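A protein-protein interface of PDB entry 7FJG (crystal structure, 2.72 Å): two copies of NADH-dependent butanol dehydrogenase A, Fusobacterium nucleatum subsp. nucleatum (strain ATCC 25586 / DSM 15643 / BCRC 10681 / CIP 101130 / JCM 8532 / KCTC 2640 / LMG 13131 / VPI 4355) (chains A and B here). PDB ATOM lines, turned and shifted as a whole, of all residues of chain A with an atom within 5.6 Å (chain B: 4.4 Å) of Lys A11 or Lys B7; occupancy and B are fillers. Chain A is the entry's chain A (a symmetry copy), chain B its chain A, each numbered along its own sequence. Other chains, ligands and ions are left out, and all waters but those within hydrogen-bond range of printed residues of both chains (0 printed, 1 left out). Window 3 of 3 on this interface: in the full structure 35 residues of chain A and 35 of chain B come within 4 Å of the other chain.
Lys A11 touches just these residues of chain B: Tyr B6 and Lys B7.
Of chain A, only Asp A9 and Lys A11 come within 4 Å of Lys B7.
Printed residues of chain A within 4 Å of Tyr B6: Thr A10, Lys A11 and Ile A12.
Of the printed residues of chain B, Ile A12 touches Asn B5 and Tyr B6.
Phe A29 touches none of the printed residues of chain B.
Phe B174 touches none of the printed residues of chain A.
The backbone NH (N) of Tyr B6 is in hydrogen-bond range of the backbone carbonyl oxygen (O) of Ile A12 (2.9 Å).
O of Asp A9 sits at hydrogen-bond distance from NZ of Lys B7 (3.0 Å).
No position is printed for both chains.
OE2 of Glu B171 is in salt-bridge range of NZ of Lys B7.
OG1 of Thr A10 lies within hydrogen-bond range of O of Pro A175, at 3.1 Å.
The side-chain amide oxygen (OD1) of Asn A25 is in hydrogen-bond range of the side-chain amino group (NZ) of Lys A11, at 2.9 Å.
N of Lys A11 is in hydrogen-bond range of O of Lys A176 (3.1 Å).
N of Ala A178 lies within hydrogen-bond range of O of Lys A11 (2.7 Å).
The backbone NH (N) of Ile A13 sits at hydrogen-bond distance from the backbone carbonyl oxygen (O) of Ala A178, 2.9 Å away.
Among the printed residues, pairs that only touch across the chains: Ile A13 with Asn B5 (3.0 Å), Ile A12 with Asn B5 (3.0 Å), Lys A11 with Tyr B6 (3.6 Å), Thr A10 with Tyr B6 (3.8 Å) and Lys A11 with Lys B7 (3.9 Å).
Of the 13 printed residues of chain A, 5 touch a printed residue of chain B.
Hydrophobic or aromatic side chains of chain A within 4 Å of the printed part of chain B: Ile A12 and Ile A13.
Among the printed residues, no Asp or Glu carboxylate lies within 4 Å of a Lys or Arg side-chain nitrogen of the other chain.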
ATOM      1  N   ASP A   9      24.347   4.489   8.677  1.00  0.00           N
ATOM      2  CA  ASP A   9      24.858   3.311   9.351  1.00  0.00           C
ATOM      3  C   ASP A   9      23.953   2.103   9.179  1.00  0.00           C
ATOM      4  O   ASP A   9      24.254   1.045   9.751  1.00  0.00           O
ATOM      5  CB  ASP A   9      25.052   3.580  10.848  1.00  0.00           C
ATOM      6  CG  ASP A   9      23.918   4.382  11.448  1.00  0.00           C
ATOM      7  OD1 ASP A   9      22.897   4.559  10.739  1.00  0.00           O
ATOM      8  OD2 ASP A   9      24.060   4.846  12.607  1.00  0.00           O
ATOM      9  N   THR A  10      22.857   2.233   8.420  1.00  0.00           N
ATOM     10  CA  THR A  10      21.966   1.103   8.224  1.00  0.00           C
ATOM     11  C   THR A  10      22.703  -0.020   7.508  1.00  0.00           C
ATOM     12  O   THR A  10      23.339   0.195   6.473  1.00  0.00           O
ATOM     13  CB  THR A  10      20.735   1.494   7.428  1.00  0.00           C
ATOM     14  OG1 THR A  10      19.920   2.379   8.195  1.00  0.00           O
ATOM     15  CG2 THR A  10      19.933   0.223   7.097  1.00  0.00           C
ATOM     16  N   LYS A  11      22.639  -1.219   8.079  1.00  0.00           N
ATOM     17  CA  LYS A  11      23.302  -2.360   7.485  1.00  0.00           C
ATOM     18  C   LYS A  11      22.447  -2.876   6.348  1.00  0.00           C
ATOM     19  O   LYS A  11      21.220  -2.971   6.463  1.00  0.00           O
ATOM     20  CB  LYS A  11      23.536  -3.460   8.510  1.00  0.00           C
ATOM     21  CG  LYS A  11      24.667  -4.415   8.141  1.00  0.00           C
ATOM     22  CD  LYS A  11      24.695  -5.622   9.048  1.00  0.00           C
ATOM     23  CE  LYS A  11      25.759  -6.628   8.633  1.00  0.00           C
ATOM     24  NZ  LYS A  11      25.585  -7.984   9.271  1.00  0.00           N
ATOM     25  N   ILE A  12      23.094  -3.145   5.225  1.00  0.00           N
ATOM     26  CA  ILE A  12      22.440  -3.657   4.032  1.00  0.00           C
ATOM     27  C   ILE A  12      22.718  -5.146   3.990  1.00  0.00           C
ATOM     28  O   ILE A  12      23.887  -5.544   3.935  1.00  0.00           O
ATOM     29  CB  ILE A  12      22.978  -2.974   2.769  1.00  0.00           C
ATOM     30  CG1 ILE A  12      22.698  -1.469   2.820  1.00  0.00           C
ATOM     31  CG2 ILE A  12      22.412  -3.677   1.544  1.00  0.00           C
ATOM     32  CD1 ILE A  12      21.382  -1.115   2.332  1.00  0.00           C
ATOM     33  N   ILE A  13      21.669  -5.976   4.042  1.00  0.00           N
ATOM     34  CA  ILE A  13      21.795  -7.403   3.718  1.00  0.00           C
ATOM     35  C   ILE A  13      21.063  -7.662   2.406  1.00  0.00           C
ATOM     36  O   ILE A  13      19.839  -7.861   2.393  1.00  0.00           O
ATOM     37  CB  ILE A  13      21.254  -8.316   4.818  1.00  0.00           C
ATOM     38  CG1 ILE A  13      22.035  -8.070   6.104  1.00  0.00           C
ATOM     39  CG2 ILE A  13      21.352  -9.735   4.354  1.00  0.00           C
ATOM     40  CD1 ILE A  13      21.242  -7.313   7.114  1.00  0.00           C
ATOM     41  N   ASN A  25      21.016 -11.317  12.485  1.00  0.00           N
ATOM     42  CA  ASN A  25      21.212  -9.894  12.667  1.00  0.00           C
ATOM     43  C   ASN A  25      20.387  -9.369  13.816  1.00  0.00           C
ATOM     44  O   ASN A  25      20.734  -8.339  14.392  1.00  0.00           O
ATOM     45  CB  ASN A  25      20.888  -9.144  11.369  1.00  0.00           C
ATOM     46  CG  ASN A  25      21.989  -9.286  10.341  1.00  0.00           C
ATOM     47  OD1 ASN A  25      23.034  -8.625  10.423  1.00  0.00           O
ATOM     48  ND2 ASN A  25      21.798 -10.211   9.406  1.00  0.00           N
ATOM     49  N   ILE A  28      22.671  -9.875  16.527  1.00  0.00           N
ATOM     50  CA  ILE A  28      23.852  -9.033  16.532  1.00  0.00           C
ATOM     51  C   ILE A  28      23.577  -7.641  17.087  1.00  0.00           C
ATOM     52  O   ILE A  28      24.493  -7.009  17.617  1.00  0.00           O
ATOM     53  CB  ILE A  28      24.460  -8.876  15.132  1.00  0.00           C
ATOM     54  CG1 ILE A  28      25.309 -10.045  14.723  1.00  0.00           C
ATOM     55  CG2 ILE A  28      25.343  -7.586  15.100  1.00  0.00           C
ATOM     56  CD1 ILE A  28      25.716  -9.925  13.265  1.00  0.00           C
ATOM     57  N   PHE A  29      22.387  -7.075  16.865  1.00  0.00           N
ATOM     58  CA  PHE A  29      22.115  -5.712  17.317  1.00  0.00           C
ATOM     59  C   PHE A  29      21.041  -5.642  18.403  1.00  0.00           C
ATOM     60  O   PHE A  29      20.468  -4.566  18.618  1.00  0.00           O
ATOM     61  CB  PHE A  29      21.737  -4.777  16.138  1.00  0.00           C
ATOM     62  CG  PHE A  29      22.603  -4.965  14.920  1.00  0.00           C
ATOM     63  CD1 PHE A  29      23.854  -4.342  14.799  1.00  0.00           C
ATOM     64  CD2 PHE A  29      22.187  -5.793  13.901  1.00  0.00           C
ATOM     65  CE1 PHE A  29      24.682  -4.577  13.667  1.00  0.00           C
ATOM     66  CE2 PHE A  29      22.992  -6.026  12.773  1.00  0.00           C
ATOM     67  CZ  PHE A  29      24.235  -5.430  12.659  1.00  0.00           C
ATOM     68  N   PRO A 175      17.559   2.309  10.746  1.00  0.00           N
ATOM     69  CA  PRO A 175      17.566   0.873  10.989  1.00  0.00           C
ATOM     70  C   PRO A 175      18.928   0.348  11.341  1.00  0.00           C
ATOM     71  O   PRO A 175      19.934   0.836  10.839  1.00  0.00           O
ATOM     72  CB  PRO A 175      17.088   0.318   9.645  1.00  0.00           C
ATOM     73  CG  PRO A 175      16.142   1.386   9.177  1.00  0.00           C
ATOM     74  CD  PRO A 175      16.418   2.602  10.057  1.00  0.00           C
ATOM     75  N   LYS A 176      18.983  -0.638  12.214  1.00  0.00           N
ATOM     76  CA  LYS A 176      20.259  -1.297  12.418  1.00  0.00           C
ATOM     77  C   LYS A 176      20.622  -2.150  11.204  1.00  0.00           C
ATOM     78  O   LYS A 176      21.804  -2.238  10.844  1.00  0.00           O
ATOM     79  CB  LYS A 176      20.191  -2.097  13.709  1.00  0.00           C
ATOM     80  CG  LYS A 176      19.678  -1.234  14.890  1.00  0.00           C
ATOM     81  CD  LYS A 176      20.468   0.061  15.005  1.00  0.00           C
ATOM     82  CE  LYS A 176      20.078   0.881  16.213  1.00  0.00           C
ATOM     83  NZ  LYS A 176      21.272   1.604  16.783  1.00  0.00           N
ATOM     84  N   PHE A 177      19.625  -2.743  10.541  1.00  0.00           N
ATOM     85  CA  PHE A 177      19.861  -3.545   9.348  1.00  0.00           C
ATOM     86  C   PHE A 177      18.578  -3.569   8.522  1.00  0.00           C
ATOM     87  O   PHE A 177      17.483  -3.295   9.020  1.00  0.00           O
ATOM     88  CB  PHE A 177      20.362  -4.963   9.692  1.00  0.00           C
ATOM     89  CG  PHE A 177      19.289  -5.906  10.186  1.00  0.00           C
ATOM     90  CD1 PHE A 177      18.440  -6.549   9.305  1.00  0.00           C
ATOM     91  CD2 PHE A 177      19.155  -6.165  11.517  1.00  0.00           C
ATOM     92  CE1 PHE A 177      17.478  -7.387   9.764  1.00  0.00           C
ATOM     93  CE2 PHE A 177      18.201  -7.004  11.962  1.00  0.00           C
ATOM     94  CZ  PHE A 177      17.364  -7.613  11.091  1.00  0.00           C
ATOM     95  N   ALA A 178      18.747  -3.834   7.226  1.00  0.00           N
ATOM     96  CA  ALA A 178      17.640  -3.936   6.284  1.00  0.00           C
ATOM     97  C   ALA A 178      17.931  -5.106   5.360  1.00  0.00           C
ATOM     98  O   ALA A 178      18.947  -5.109   4.660  1.00  0.00           O
ATOM     99  CB  ALA A 178      17.466  -2.648   5.485  1.00  0.00           C
ATOM    100  N   ILE A 179      17.076  -6.119   5.424  1.00  0.00           N
ATOM    101  CA  ILE A 179      17.144  -7.240   4.495  1.00  0.00           C
ATOM    102  C   ILE A 179      16.535  -6.791   3.173  1.00  0.00           C
ATOM    103  O   ILE A 179      15.404  -6.282   3.136  1.00  0.00           O
ATOM    104  CB  ILE A 179      16.407  -8.477   5.052  1.00  0.00           C
ATOM    105  CG1 ILE A 179      17.018  -8.963   6.378  1.00  0.00           C
ATOM    106  CG2 ILE A 179      16.397  -9.587   3.956  1.00  0.00           C
ATOM    107  CD1 ILE A 179      18.323  -9.720   6.181  1.00  0.00           C
ATOM    108  N   ASN B   5      26.700  -7.909   1.857  1.00  0.00           N
ATOM    109  CA  ASN B   5      26.374  -6.991   2.940  1.00  0.00           C
ATOM    110  C   ASN B   5      27.177  -5.691   2.833  1.00  0.00           C
ATOM    111  O   ASN B   5      28.248  -5.637   2.223  1.00  0.00           O
ATOM    112  CB  ASN B   5      26.617  -7.655   4.304  1.00  0.00           C
ATOM    113  CG  ASN B   5      25.774  -8.888   4.492  1.00  0.00           C
ATOM    114  OD1 ASN B   5      24.732  -8.851   5.135  1.00  0.00           O
ATOM    115  ND2 ASN B   5      26.206  -9.987   3.911  1.00  0.00           N
ATOM    116  N   TYR B   6      26.629  -4.616   3.400  1.00  0.00           N
ATOM    117  CA  TYR B   6      27.362  -3.354   3.412  1.00  0.00           C
ATOM    118  C   TYR B   6      27.068  -2.536   4.657  1.00  0.00           C
ATOM    119  O   TYR B   6      25.909  -2.198   4.936  1.00  0.00           O
ATOM    120  CB  TYR B   6      27.050  -2.522   2.178  1.00  0.00           C
ATOM    121  CG  TYR B   6      27.556  -1.093   2.277  1.00  0.00           C
ATOM    122  CD1 TYR B   6      28.894  -0.784   1.996  1.00  0.00           C
ATOM    123  CD2 TYR B   6      26.703  -0.055   2.651  1.00  0.00           C
ATOM    124  CE1 TYR B   6      29.365   0.505   2.089  1.00  0.00           C
ATOM    125  CE2 TYR B   6      27.162   1.244   2.733  1.00  0.00           C
ATOM    126  CZ  TYR B   6      28.492   1.528   2.450  1.00  0.00           C
ATOM    127  OH  TYR B   6      28.932   2.847   2.544  1.00  0.00           O
ATOM    128  N   LYS B   7      28.139  -2.173   5.362  1.00  0.00           N
ATOM    129  CA  LYS B   7      28.078  -1.218   6.457  1.00  0.00           C
ATOM    130  C   LYS B   7      29.191  -0.198   6.289  1.00  0.00           C
ATOM    131  O   LYS B   7      30.293  -0.526   5.825  1.00  0.00           O
ATOM    132  CB  LYS B   7      28.227  -1.912   7.787  1.00  0.00           C
ATOM    133  CG  LYS B   7      27.500  -1.272   8.930  1.00  0.00           C
ATOM    134  CD  LYS B   7      27.363  -2.290  10.095  1.00  0.00           C
ATOM    135  CE  LYS B   7      27.252  -1.606  11.466  1.00  0.00           C
ATOM    136  NZ  LYS B   7      26.276  -0.472  11.411  1.00  0.00           N
ATOM    137  N   ASN B   8      28.889   1.040   6.654  1.00  0.00           N
ATOM    138  CA  ASN B   8      29.931   2.040   6.843  1.00  0.00           C
ATOM    139  C   ASN B   8      29.353   3.253   7.555  1.00  0.00           C
ATOM    140  O   ASN B   8      28.594   4.037   6.973  1.00  0.00           O
ATOM    141  CB  ASN B   8      30.561   2.446   5.517  1.00  0.00           C
ATOM    142  CG  ASN B   8      31.829   3.234   5.713  1.00  0.00           C
ATOM    143  OD1 ASN B   8      31.807   4.339   6.267  1.00  0.00           O
ATOM    144  ND2 ASN B   8      32.950   2.668   5.292  1.00  0.00           N
ATOM    145  N   GLU B 171      34.503  -3.862  12.676  1.00  0.00           N
ATOM    146  CA  GLU B 171      33.612  -2.728  12.525  1.00  0.00           C
ATOM    147  C   GLU B 171      33.801  -1.659  13.596  1.00  0.00           C
ATOM    148  O   GLU B 171      33.188  -0.579  13.494  1.00  0.00           O
ATOM    149  CB  GLU B 171      32.171  -3.220  12.543  1.00  0.00           C
ATOM    150  CG  GLU B 171      31.162  -2.128  12.251  1.00  0.00           C
ATOM    151  CD  GLU B 171      30.066  -2.105  13.273  1.00  0.00           C
ATOM    152  OE1 GLU B 171      29.836  -3.192  13.852  1.00  0.00           O
ATOM    153  OE2 GLU B 171      29.458  -1.028  13.519  1.00  0.00           O
ATOM    154  N   PHE B 174      35.986   1.738  12.418  1.00  0.00           N
ATOM    155  CA  PHE B 174      35.370   2.807  11.654  1.00  0.00           C
ATOM    156  C   PHE B 174      35.419   4.140  12.397  1.00  0.00           C
ATOM    157  O   PHE B 174      34.732   4.323  13.417  1.00  0.00           O
ATOM    158  CB  PHE B 174      33.911   2.477  11.329  1.00  0.00           C
ATOM    159  CG  PHE B 174      33.725   1.561  10.176  1.00  0.00           C
ATOM    160  CD1 PHE B 174      34.621   1.538   9.117  1.00  0.00           C
ATOM    161  CD2 PHE B 174      32.630   0.707  10.139  1.00  0.00           C
ATOM    162  CE1 PHE B 174      34.430   0.684   8.042  1.00  0.00           C
ATOM    163  CE2 PHE B 174      32.435  -0.164   9.068  1.00  0.00           C
ATOM    164  CZ  PHE B 174      33.335  -0.168   8.022  1.00  0.00           C
